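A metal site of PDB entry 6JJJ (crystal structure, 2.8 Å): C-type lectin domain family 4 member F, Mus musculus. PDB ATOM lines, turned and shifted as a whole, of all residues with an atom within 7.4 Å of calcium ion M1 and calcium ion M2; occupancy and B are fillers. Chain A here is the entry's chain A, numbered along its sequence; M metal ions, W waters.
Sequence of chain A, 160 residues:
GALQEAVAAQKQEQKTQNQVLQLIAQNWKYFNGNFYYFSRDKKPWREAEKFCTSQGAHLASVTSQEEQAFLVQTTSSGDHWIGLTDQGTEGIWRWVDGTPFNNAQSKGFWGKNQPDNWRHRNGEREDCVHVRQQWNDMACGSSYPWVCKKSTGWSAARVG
The side-chain carboxylate (OE1) of Glu 126 lies close to the backbone NH (N) of Trp 118, 3.1 Å away.
O of Met 138 is in hydrogen-bond range of N of Asp 127, 3.1 Å away.
The side-chain amide oxygen (OD1) of Asn 136 sits close to the side-chain amide nitrogen (NE2) of Gln 114 (2.8 Å).
N of Asn 136 is in hydrogen-bond range of O of His 130 (3.2 Å).
The side-chain amide oxygen (OE1) of Gln 114 sits at hydrogen-bond distance from the backbone NH (N) of Asp 116 (2.4 Å).
The side-chain carboxylate (OD1) of Asp 116 lies close to the backbone NH (N) of Trp 118 (3.4 Å).
N of Asn 117 is in hydrogen-bond range of OD2 of Asp 137, at 2.8 Å.
The side-chain amide oxygen (OE1) of Gln 114 sits close to the side-chain carboxylate (OD1) of Asp 137, at 3.0 Å.
Gln 114 touches calcium ion M1 (OE1 to CA, 3.4 Å).
Calcium ion M1 is bound by the side-chain carboxylate of Glu 126, water W1, the side-chain amide oxygen of Asn 136, the side-chain carboxylate of Asp 116, the backbone carbonyl oxygen of Asp 137 and the side-chain carboxylate of Asp 137.
Calcium ion M1 has six donor atoms within binding distance.
Slightly farther from calcium ion M1 lies OE2 of Glu 126 (3.0 Å).
Slightly farther from calcium ion M1 lies the side-chain carboxylate (OD2) of Asp 116 (3.1 Å).
Calcium ion M2 is bound by the side-chain carboxylate (OE2) of Glu 90 (2.1 Å), the side-chain carboxylate (OD1) of Asp 86 (2.3 Å), the side-chain carboxylate (OD1) of Asp 127 (2.3 Å), the side-chain carboxylate (OD2) of Asp 86 (2.3 Å), the backbone carbonyl oxygen (O) of Glu 126 (2.4 Å) and the side-chain amide oxygen (OD1) of Asn 117 (2.8 Å).
Calcium ion M2 has six donor atoms within binding distance.
Slightly farther from calcium ion M2 lies OE1 of Glu 90 (3.0 Å).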
ATOM      1  N   THR A  85      -7.322 -19.322 -11.173  1.00  0.00           N
ATOM      2  CA  THR A  85      -6.683 -18.091 -10.748  1.00  0.00           C
ATOM      3  C   THR A  85      -5.399 -18.394  -9.995  1.00  0.00           C
ATOM      4  O   THR A  85      -5.305 -19.395  -9.279  1.00  0.00           O
ATOM      5  CB  THR A  85      -7.622 -17.246  -9.871  1.00  0.00           C
ATOM      6  OG1 THR A  85      -6.894 -16.125  -9.335  1.00  0.00           O
ATOM      7  CG2 THR A  85      -8.184 -18.082  -8.734  1.00  0.00           C
ATOM      8  N   ASP A  86      -4.423 -17.497 -10.132  1.00  0.00           N
ATOM      9  CA  ASP A  86      -3.160 -17.538  -9.403  1.00  0.00           C
ATOM     10  C   ASP A  86      -3.087 -16.296  -8.503  1.00  0.00           C
ATOM     11  O   ASP A  86      -2.042 -15.683  -8.321  1.00  0.00           O
ATOM     12  CB  ASP A  86      -1.960 -17.609 -10.338  1.00  0.00           C
ATOM     13  CG  ASP A  86      -1.777 -16.349 -11.168  1.00  0.00           C
ATOM     14  OD1 ASP A  86      -2.642 -15.451 -11.099  1.00  0.00           O
ATOM     15  OD2 ASP A  86      -0.760 -16.267 -11.891  1.00  0.00           O
ATOM     16  N   GLN A  87      -4.227 -15.921  -7.950  1.00  0.00           N
ATOM     17  CA  GLN A  87      -4.366 -14.743  -7.106  1.00  0.00           C
ATOM     18  C   GLN A  87      -3.559 -14.851  -5.822  1.00  0.00           C
ATOM     19  O   GLN A  87      -2.499 -14.230  -5.732  1.00  0.00           O
ATOM     20  CB  GLN A  87      -5.843 -14.552  -6.831  1.00  0.00           C
ATOM     21  CG  GLN A  87      -6.236 -13.397  -5.954  1.00  0.00           C
ATOM     22  CD  GLN A  87      -7.744 -13.305  -5.832  1.00  0.00           C
ATOM     23  OE1 GLN A  87      -8.343 -12.329  -6.269  1.00  0.00           O
ATOM     24  NE2 GLN A  87      -8.358 -14.348  -5.282  1.00  0.00           N
ATOM     25  N   THR A  89      -1.096 -16.583  -4.682  1.00  0.00           N
ATOM     26  CA  THR A  89       0.315 -16.412  -5.039  1.00  0.00           C
ATOM     27  C   THR A  89       0.432 -16.407  -6.556  1.00  0.00           C
ATOM     28  O   THR A  89      -0.178 -17.239  -7.229  1.00  0.00           O
ATOM     29  CB  THR A  89       1.195 -17.512  -4.447  1.00  0.00           C
ATOM     30  OG1 THR A  89       1.343 -18.567  -5.399  1.00  0.00           O
ATOM     31  CG2 THR A  89       0.582 -18.066  -3.177  1.00  0.00           C
ATOM     32  N   GLU A  90       1.227 -15.473  -7.086  1.00  0.00           N
ATOM     33  CA  GLU A  90       1.277 -15.263  -8.527  1.00  0.00           C
ATOM     34  C   GLU A  90       1.687 -16.517  -9.286  1.00  0.00           C
ATOM     35  O   GLU A  90       1.347 -16.660 -10.471  1.00  0.00           O
ATOM     36  CB  GLU A  90       2.232 -14.123  -8.850  1.00  0.00           C
ATOM     37  CG  GLU A  90       2.289 -13.767 -10.315  1.00  0.00           C
ATOM     38  CD  GLU A  90       0.927 -13.459 -10.883  1.00  0.00           C
ATOM     39  OE1 GLU A  90       0.074 -12.930 -10.147  1.00  0.00           O
ATOM     40  OE2 GLU A  90       0.712 -13.763 -12.075  1.00  0.00           O
ATOM     41  N   GLY A  91       2.418 -17.417  -8.648  1.00  0.00           N
ATOM     42  CA  GLY A  91       2.902 -18.594  -9.340  1.00  0.00           C
ATOM     43  C   GLY A  91       1.869 -19.692  -9.473  1.00  0.00           C
ATOM     44  O   GLY A  91       1.564 -20.125 -10.589  1.00  0.00           O
ATOM     45  N   ILE A  92       1.323 -20.125  -8.351  1.00  0.00           N
ATOM     46  CA  ILE A  92       0.451 -21.308  -8.343  1.00  0.00           C
ATOM     47  C   ILE A  92      -0.940 -20.895  -8.797  1.00  0.00           C
ATOM     48  O   ILE A  92      -1.504 -19.915  -8.308  1.00  0.00           O
ATOM     49  CB  ILE A  92       0.422 -21.941  -6.943  1.00  0.00           C
ATOM     50  CG1 ILE A  92      -0.440 -21.092  -5.991  1.00  0.00           C
ATOM     51  CG2 ILE A  92       1.832 -22.105  -6.403  1.00  0.00           C
ATOM     52  CD1 ILE A  92      -0.352 -21.498  -4.537  1.00  0.00           C
ATOM     53  N   TRP A  93      -1.493 -21.664  -9.727  1.00  0.00           N
ATOM     54  CA  TRP A  93      -2.904 -21.592 -10.075  1.00  0.00           C
ATOM     55  C   TRP A  93      -3.658 -22.638  -9.265  1.00  0.00           C
ATOM     56  O   TRP A  93      -3.085 -23.589  -8.743  1.00  0.00           O
ATOM     57  CB  TRP A  93      -3.125 -21.845 -11.567  1.00  0.00           C
ATOM     58  CG  TRP A  93      -2.399 -20.881 -12.461  1.00  0.00           C
ATOM     59  CD1 TRP A  93      -1.137 -21.025 -12.952  1.00  0.00           C
ATOM     60  CD2 TRP A  93      -2.913 -19.658 -13.004  1.00  0.00           C
ATOM     61  NE1 TRP A  93      -0.818 -19.950 -13.759  1.00  0.00           N
ATOM     62  CE2 TRP A  93      -1.895 -19.099 -13.808  1.00  0.00           C
ATOM     63  CE3 TRP A  93      -4.124 -18.973 -12.888  1.00  0.00           C
ATOM     64  CZ2 TRP A  93      -2.050 -17.895 -14.477  1.00  0.00           C
ATOM     65  CZ3 TRP A  93      -4.277 -17.779 -13.565  1.00  0.00           C
ATOM     66  CH2 TRP A  93      -3.246 -17.256 -14.348  1.00  0.00           C
ATOM     67  N   ASN A 113       1.122 -18.671 -26.435  1.00  0.00           N
ATOM     68  CA  ASN A 113       2.024 -18.145 -25.417  1.00  0.00           C
ATOM     69  C   ASN A 113       1.137 -17.566 -24.311  1.00  0.00           C
ATOM     70  O   ASN A 113       0.767 -16.385 -24.352  1.00  0.00           O
ATOM     71  CB  ASN A 113       3.004 -17.111 -25.984  1.00  0.00           C
ATOM     72  CG  ASN A 113       2.330 -16.010 -26.776  1.00  0.00           C
ATOM     73  OD1 ASN A 113       1.866 -15.018 -26.204  1.00  0.00           O
ATOM     74  ND2 ASN A 113       2.280 -16.172 -28.089  1.00  0.00           N
ATOM     75  N   GLN A 114       0.776 -18.402 -23.330  1.00  0.00           N
ATOM     76  CA  GLN A 114      -0.163 -18.024 -22.284  1.00  0.00           C
ATOM     77  C   GLN A 114      -0.011 -19.022 -21.147  1.00  0.00           C
ATOM     78  O   GLN A 114       0.227 -20.205 -21.422  1.00  0.00           O
ATOM     79  CB  GLN A 114      -1.604 -18.030 -22.809  1.00  0.00           C
ATOM     80  CG  GLN A 114      -2.554 -17.038 -22.158  1.00  0.00           C
ATOM     81  CD  GLN A 114      -2.067 -15.609 -22.243  1.00  0.00           C
ATOM     82  OE1 GLN A 114      -1.334 -15.138 -21.369  1.00  0.00           O
ATOM     83  NE2 GLN A 114      -2.473 -14.899 -23.293  1.00  0.00           N
ATOM     84  N   PRO A 115      -0.134 -18.605 -19.878  1.00  0.00           N
ATOM     85  CA  PRO A 115      -0.436 -17.245 -19.395  1.00  0.00           C
ATOM     86  C   PRO A 115       0.731 -16.264 -19.536  1.00  0.00           C
ATOM     87  O   PRO A 115       1.892 -16.672 -19.492  1.00  0.00           O
ATOM     88  CB  PRO A 115      -0.766 -17.465 -17.910  1.00  0.00           C
ATOM     89  CG  PRO A 115       0.010 -18.696 -17.536  1.00  0.00           C
ATOM     90  CD  PRO A 115       0.021 -19.564 -18.763  1.00  0.00           C
ATOM     91  N   ASP A 116       0.403 -14.981 -19.698  1.00  0.00           N
ATOM     92  CA  ASP A 116       1.404 -13.932 -19.810  1.00  0.00           C
ATOM     93  C   ASP A 116       1.428 -13.005 -18.610  1.00  0.00           C
ATOM     94  O   ASP A 116       2.456 -12.351 -18.369  1.00  0.00           O
ATOM     95  CB  ASP A 116       1.175 -13.102 -21.073  1.00  0.00           C
ATOM     96  CG  ASP A 116      -0.212 -12.501 -21.133  1.00  0.00           C
ATOM     97  OD1 ASP A 116      -1.015 -12.786 -20.222  1.00  0.00           O
ATOM     98  OD2 ASP A 116      -0.510 -11.759 -22.091  1.00  0.00           O
ATOM     99  N   ASN A 117       0.334 -12.928 -17.847  1.00  0.00           N
ATOM    100  CA  ASN A 117       0.261 -12.053 -16.672  1.00  0.00           C
ATOM    101  C   ASN A 117       0.488 -10.599 -17.075  1.00  0.00           C
ATOM    102  O   ASN A 117       1.234  -9.858 -16.413  1.00  0.00           O
ATOM    103  CB  ASN A 117       1.256 -12.489 -15.594  1.00  0.00           C
ATOM    104  CG  ASN A 117       0.863 -11.998 -14.224  1.00  0.00           C
ATOM    105  OD1 ASN A 117      -0.317 -11.934 -13.896  1.00  0.00           O
ATOM    106  ND2 ASN A 117       1.861 -11.662 -13.404  1.00  0.00           N
ATOM    107  N   TRP A 118      -0.142 -10.191 -18.158  1.00  0.00           N
ATOM    108  CA  TRP A 118       0.082  -8.864 -18.720  1.00  0.00           C
ATOM    109  C   TRP A 118      -0.269  -7.787 -17.701  1.00  0.00           C
ATOM    110  O   TRP A 118      -1.166  -7.960 -16.872  1.00  0.00           O
ATOM    111  CB  TRP A 118      -0.756  -8.688 -19.990  1.00  0.00           C
ATOM    112  CG  TRP A 118      -0.326  -7.557 -20.851  1.00  0.00           C
ATOM    113  CD1 TRP A 118       0.835  -7.458 -21.566  1.00  0.00           C
ATOM    114  CD2 TRP A 118      -1.053  -6.357 -21.126  1.00  0.00           C
ATOM    115  NE1 TRP A 118       0.878  -6.275 -22.258  1.00  0.00           N
ATOM    116  CE2 TRP A 118      -0.274  -5.575 -22.006  1.00  0.00           C
ATOM    117  CE3 TRP A 118      -2.300  -5.870 -20.712  1.00  0.00           C
ATOM    118  CZ2 TRP A 118      -0.695  -4.334 -22.465  1.00  0.00           C
ATOM    119  CZ3 TRP A 118      -2.710  -4.629 -21.179  1.00  0.00           C
ATOM    120  CH2 TRP A 118      -1.913  -3.877 -22.043  1.00  0.00           C
ATOM    121  N   HIS A 120      -1.957  -4.469 -16.929  1.00  0.00           N
ATOM    122  CA  HIS A 120      -2.974  -3.604 -17.505  1.00  0.00           C
ATOM    123  C   HIS A 120      -2.754  -2.152 -17.080  1.00  0.00           C
ATOM    124  O   HIS A 120      -2.027  -1.853 -16.129  1.00  0.00           O
ATOM    125  CB  HIS A 120      -4.368  -4.066 -17.093  1.00  0.00           C
ATOM    126  CG  HIS A 120      -4.899  -5.207 -17.904  1.00  0.00           C
ATOM    127  ND1 HIS A 120      -5.947  -5.080 -18.789  1.00  0.00           N
ATOM    128  CD2 HIS A 120      -4.499  -6.502 -17.986  1.00  0.00           C
ATOM    129  CE1 HIS A 120      -6.187  -6.237 -19.361  1.00  0.00           C
ATOM    130  NE2 HIS A 120      -5.315  -7.125 -18.896  1.00  0.00           N
ATOM    131  N   ARG A 125      -2.485  -6.707 -12.698  1.00  0.00           N
ATOM    132  CA  ARG A 125      -1.894  -7.826 -13.415  1.00  0.00           C
ATOM    133  C   ARG A 125      -3.047  -8.717 -13.885  1.00  0.00           C
ATOM    134  O   ARG A 125      -4.212  -8.316 -13.858  1.00  0.00           O
ATOM    135  CB  ARG A 125      -0.915  -8.573 -12.514  1.00  0.00           C
ATOM    136  CG  ARG A 125       0.245  -7.721 -12.030  1.00  0.00           C
ATOM    137  CD  ARG A 125       1.102  -7.193 -13.168  1.00  0.00           C
ATOM    138  NE  ARG A 125       2.376  -6.683 -12.658  1.00  0.00           N
ATOM    139  CZ  ARG A 125       2.548  -5.460 -12.163  1.00  0.00           C
ATOM    140  NH1 ARG A 125       1.530  -4.622 -12.089  1.00  0.00           N
ATOM    141  NH2 ARG A 125       3.745  -5.083 -11.744  1.00  0.00           N
ATOM    142  N   GLU A 126      -2.746  -9.944 -14.315  1.00  0.00           N
ATOM    143  CA  GLU A 126      -3.775 -10.891 -14.752  1.00  0.00           C
ATOM    144  C   GLU A 126      -3.759 -12.107 -13.847  1.00  0.00           C
ATOM    145  O   GLU A 126      -2.784 -12.863 -13.840  1.00  0.00           O
ATOM    146  CB  GLU A 126      -3.557 -11.280 -16.209  1.00  0.00           C
ATOM    147  CG  GLU A 126      -3.678 -10.112 -17.188  1.00  0.00           C
ATOM    148  CD  GLU A 126      -3.617 -10.566 -18.633  1.00  0.00           C
ATOM    149  OE1 GLU A 126      -2.875 -11.528 -18.913  1.00  0.00           O
ATOM    150  OE2 GLU A 126      -4.315  -9.963 -19.476  1.00  0.00           O
ATOM    151  N   ASP A 127      -4.839 -12.283 -13.072  1.00  0.00           N
ATOM    152  CA  ASP A 127      -4.946 -13.402 -12.128  1.00  0.00           C
ATOM    153  C   ASP A 127      -6.263 -14.160 -12.283  1.00  0.00           C
ATOM    154  O   ASP A 127      -6.664 -14.880 -11.358  1.00  0.00           O
ATOM    155  CB  ASP A 127      -4.795 -12.915 -10.690  1.00  0.00           C
ATOM    156  CG  ASP A 127      -3.468 -12.258 -10.438  1.00  0.00           C
ATOM    157  OD1 ASP A 127      -2.473 -12.661 -11.074  1.00  0.00           O
ATOM    158  OD2 ASP A 127      -3.410 -11.343  -9.588  1.00  0.00           O
ATOM    159  N   CYS A 128      -6.958 -14.002 -13.407  1.00  0.00           N
ATOM    160  CA  CYS A 128      -8.221 -14.685 -13.639  1.00  0.00           C
ATOM    161  C   CYS A 128      -8.245 -15.156 -15.081  1.00  0.00           C
ATOM    162  O   CYS A 128      -7.667 -14.524 -15.968  1.00  0.00           O
ATOM    163  CB  CYS A 128      -9.411 -13.774 -13.333  1.00  0.00           C
ATOM    164  SG  CYS A 128      -9.627 -13.415 -11.558  1.00  0.00           S
ATOM    165  N   HIS A 130     -10.374 -16.670 -18.495  1.00  0.00           N
ATOM    166  CA  HIS A 130     -11.591 -16.836 -19.270  1.00  0.00           C
ATOM    167  C   HIS A 130     -11.269 -17.701 -20.494  1.00  0.00           C
ATOM    168  O   HIS A 130     -10.111 -18.041 -20.747  1.00  0.00           O
ATOM    169  CB  HIS A 130     -12.192 -15.484 -19.684  1.00  0.00           C
ATOM    170  CG  HIS A 130     -11.281 -14.612 -20.491  1.00  0.00           C
ATOM    171  ND1 HIS A 130     -11.422 -13.246 -20.549  1.00  0.00           N
ATOM    172  CD2 HIS A 130     -10.227 -14.915 -21.285  1.00  0.00           C
ATOM    173  CE1 HIS A 130     -10.493 -12.742 -21.329  1.00  0.00           C
ATOM    174  NE2 HIS A 130      -9.750 -13.732 -21.794  1.00  0.00           N
ATOM    175  N   TRP A 135      -7.571 -21.012 -23.027  1.00  0.00           N
ATOM    176  CA  TRP A 135      -7.553 -20.176 -21.844  1.00  0.00           C
ATOM    177  C   TRP A 135      -6.698 -18.932 -22.056  1.00  0.00           C
ATOM    178  O   TRP A 135      -5.797 -18.900 -22.896  1.00  0.00           O
ATOM    179  CB  TRP A 135      -7.015 -20.944 -20.646  1.00  0.00           C
ATOM    180  CG  TRP A 135      -7.796 -22.157 -20.303  1.00  0.00           C
ATOM    181  CD1 TRP A 135      -8.991 -22.532 -20.844  1.00  0.00           C
ATOM    182  CD2 TRP A 135      -7.456 -23.149 -19.342  1.00  0.00           C
ATOM    183  NE1 TRP A 135      -9.408 -23.710 -20.273  1.00  0.00           N
ATOM    184  CE2 TRP A 135      -8.490 -24.102 -19.348  1.00  0.00           C
ATOM    185  CE3 TRP A 135      -6.378 -23.315 -18.473  1.00  0.00           C
ATOM    186  CZ2 TRP A 135      -8.470 -25.223 -18.520  1.00  0.00           C
ATOM    187  CZ3 TRP A 135      -6.365 -24.428 -17.643  1.00  0.00           C
ATOM    188  CH2 TRP A 135      -7.403 -25.366 -17.668  1.00  0.00           C
ATOM    189  N   ASN A 136      -7.009 -17.885 -21.289  1.00  0.00           N
ATOM    190  CA  ASN A 136      -6.172 -16.695 -21.237  1.00  0.00           C
ATOM    191  C   ASN A 136      -6.338 -16.070 -19.856  1.00  0.00           C
ATOM    192  O   ASN A 136      -7.473 -15.824 -19.427  1.00  0.00           O
ATOM    193  CB  ASN A 136      -6.543 -15.676 -22.321  1.00  0.00           C
ATOM    194  CG  ASN A 136      -5.867 -14.336 -22.124  1.00  0.00           C
ATOM    195  OD1 ASN A 136      -4.693 -14.269 -21.744  1.00  0.00           O
ATOM    196  ND2 ASN A 136      -6.599 -13.254 -22.361  1.00  0.00           N
ATOM    197  N   ASP A 137      -5.231 -15.826 -19.161  1.00  0.00           N
ATOM    198  CA  ASP A 137      -5.299 -15.115 -17.893  1.00  0.00           C
ATOM    199  C   ASP A 137      -5.618 -13.648 -18.167  1.00  0.00           C
ATOM    200  O   ASP A 137      -5.177 -13.077 -19.164  1.00  0.00           O
ATOM    201  CB  ASP A 137      -4.016 -15.285 -17.088  1.00  0.00           C
ATOM    202  CG  ASP A 137      -2.827 -14.578 -17.703  1.00  0.00           C
ATOM    203  OD1 ASP A 137      -2.826 -14.324 -18.932  1.00  0.00           O
ATOM    204  OD2 ASP A 137      -1.889 -14.276 -16.944  1.00  0.00           O
ATOM    205  N   MET A 138      -6.400 -13.037 -17.284  1.00  0.00           N
ATOM    206  CA  MET A 138      -6.992 -11.740 -17.557  1.00  0.00           C
ATOM    207  C   MET A 138      -7.103 -10.950 -16.259  1.00  0.00           C
ATOM    208  O   MET A 138      -7.070 -11.520 -15.160  1.00  0.00           O
ATOM    209  CB  MET A 138      -8.375 -11.918 -18.210  1.00  0.00           C
ATOM    210  CG  MET A 138      -9.096 -10.627 -18.533  1.00  0.00           C
ATOM    211  SD  MET A 138      -8.144  -9.624 -19.701  1.00  0.00           S
ATOM    212  CE  MET A 138      -9.057  -8.081 -19.644  1.00  0.00           C
ATOM    213  N   ALA A 139      -7.230  -9.637 -16.406  1.00  0.00           N
ATOM    214  CA  ALA A 139      -7.459  -8.775 -15.246  1.00  0.00           C
ATOM    215  C   ALA A 139      -8.816  -9.098 -14.638  1.00  0.00           C
ATOM    216  O   ALA A 139      -9.840  -9.098 -15.317  1.00  0.00           O
ATOM    217  CB  ALA A 139      -7.406  -7.309 -15.664  1.00  0.00           C
HETATM  218 CA    CA M   1      -3.347 -12.409 -20.905  1.00  0.00          CA
HETATM  219 CA    CA M   2      -1.368 -14.128 -12.431  1.00  0.00          CA
HETATM  220  O   HOH W   1      -3.300 -11.305 -22.899  1.00  0.00           O
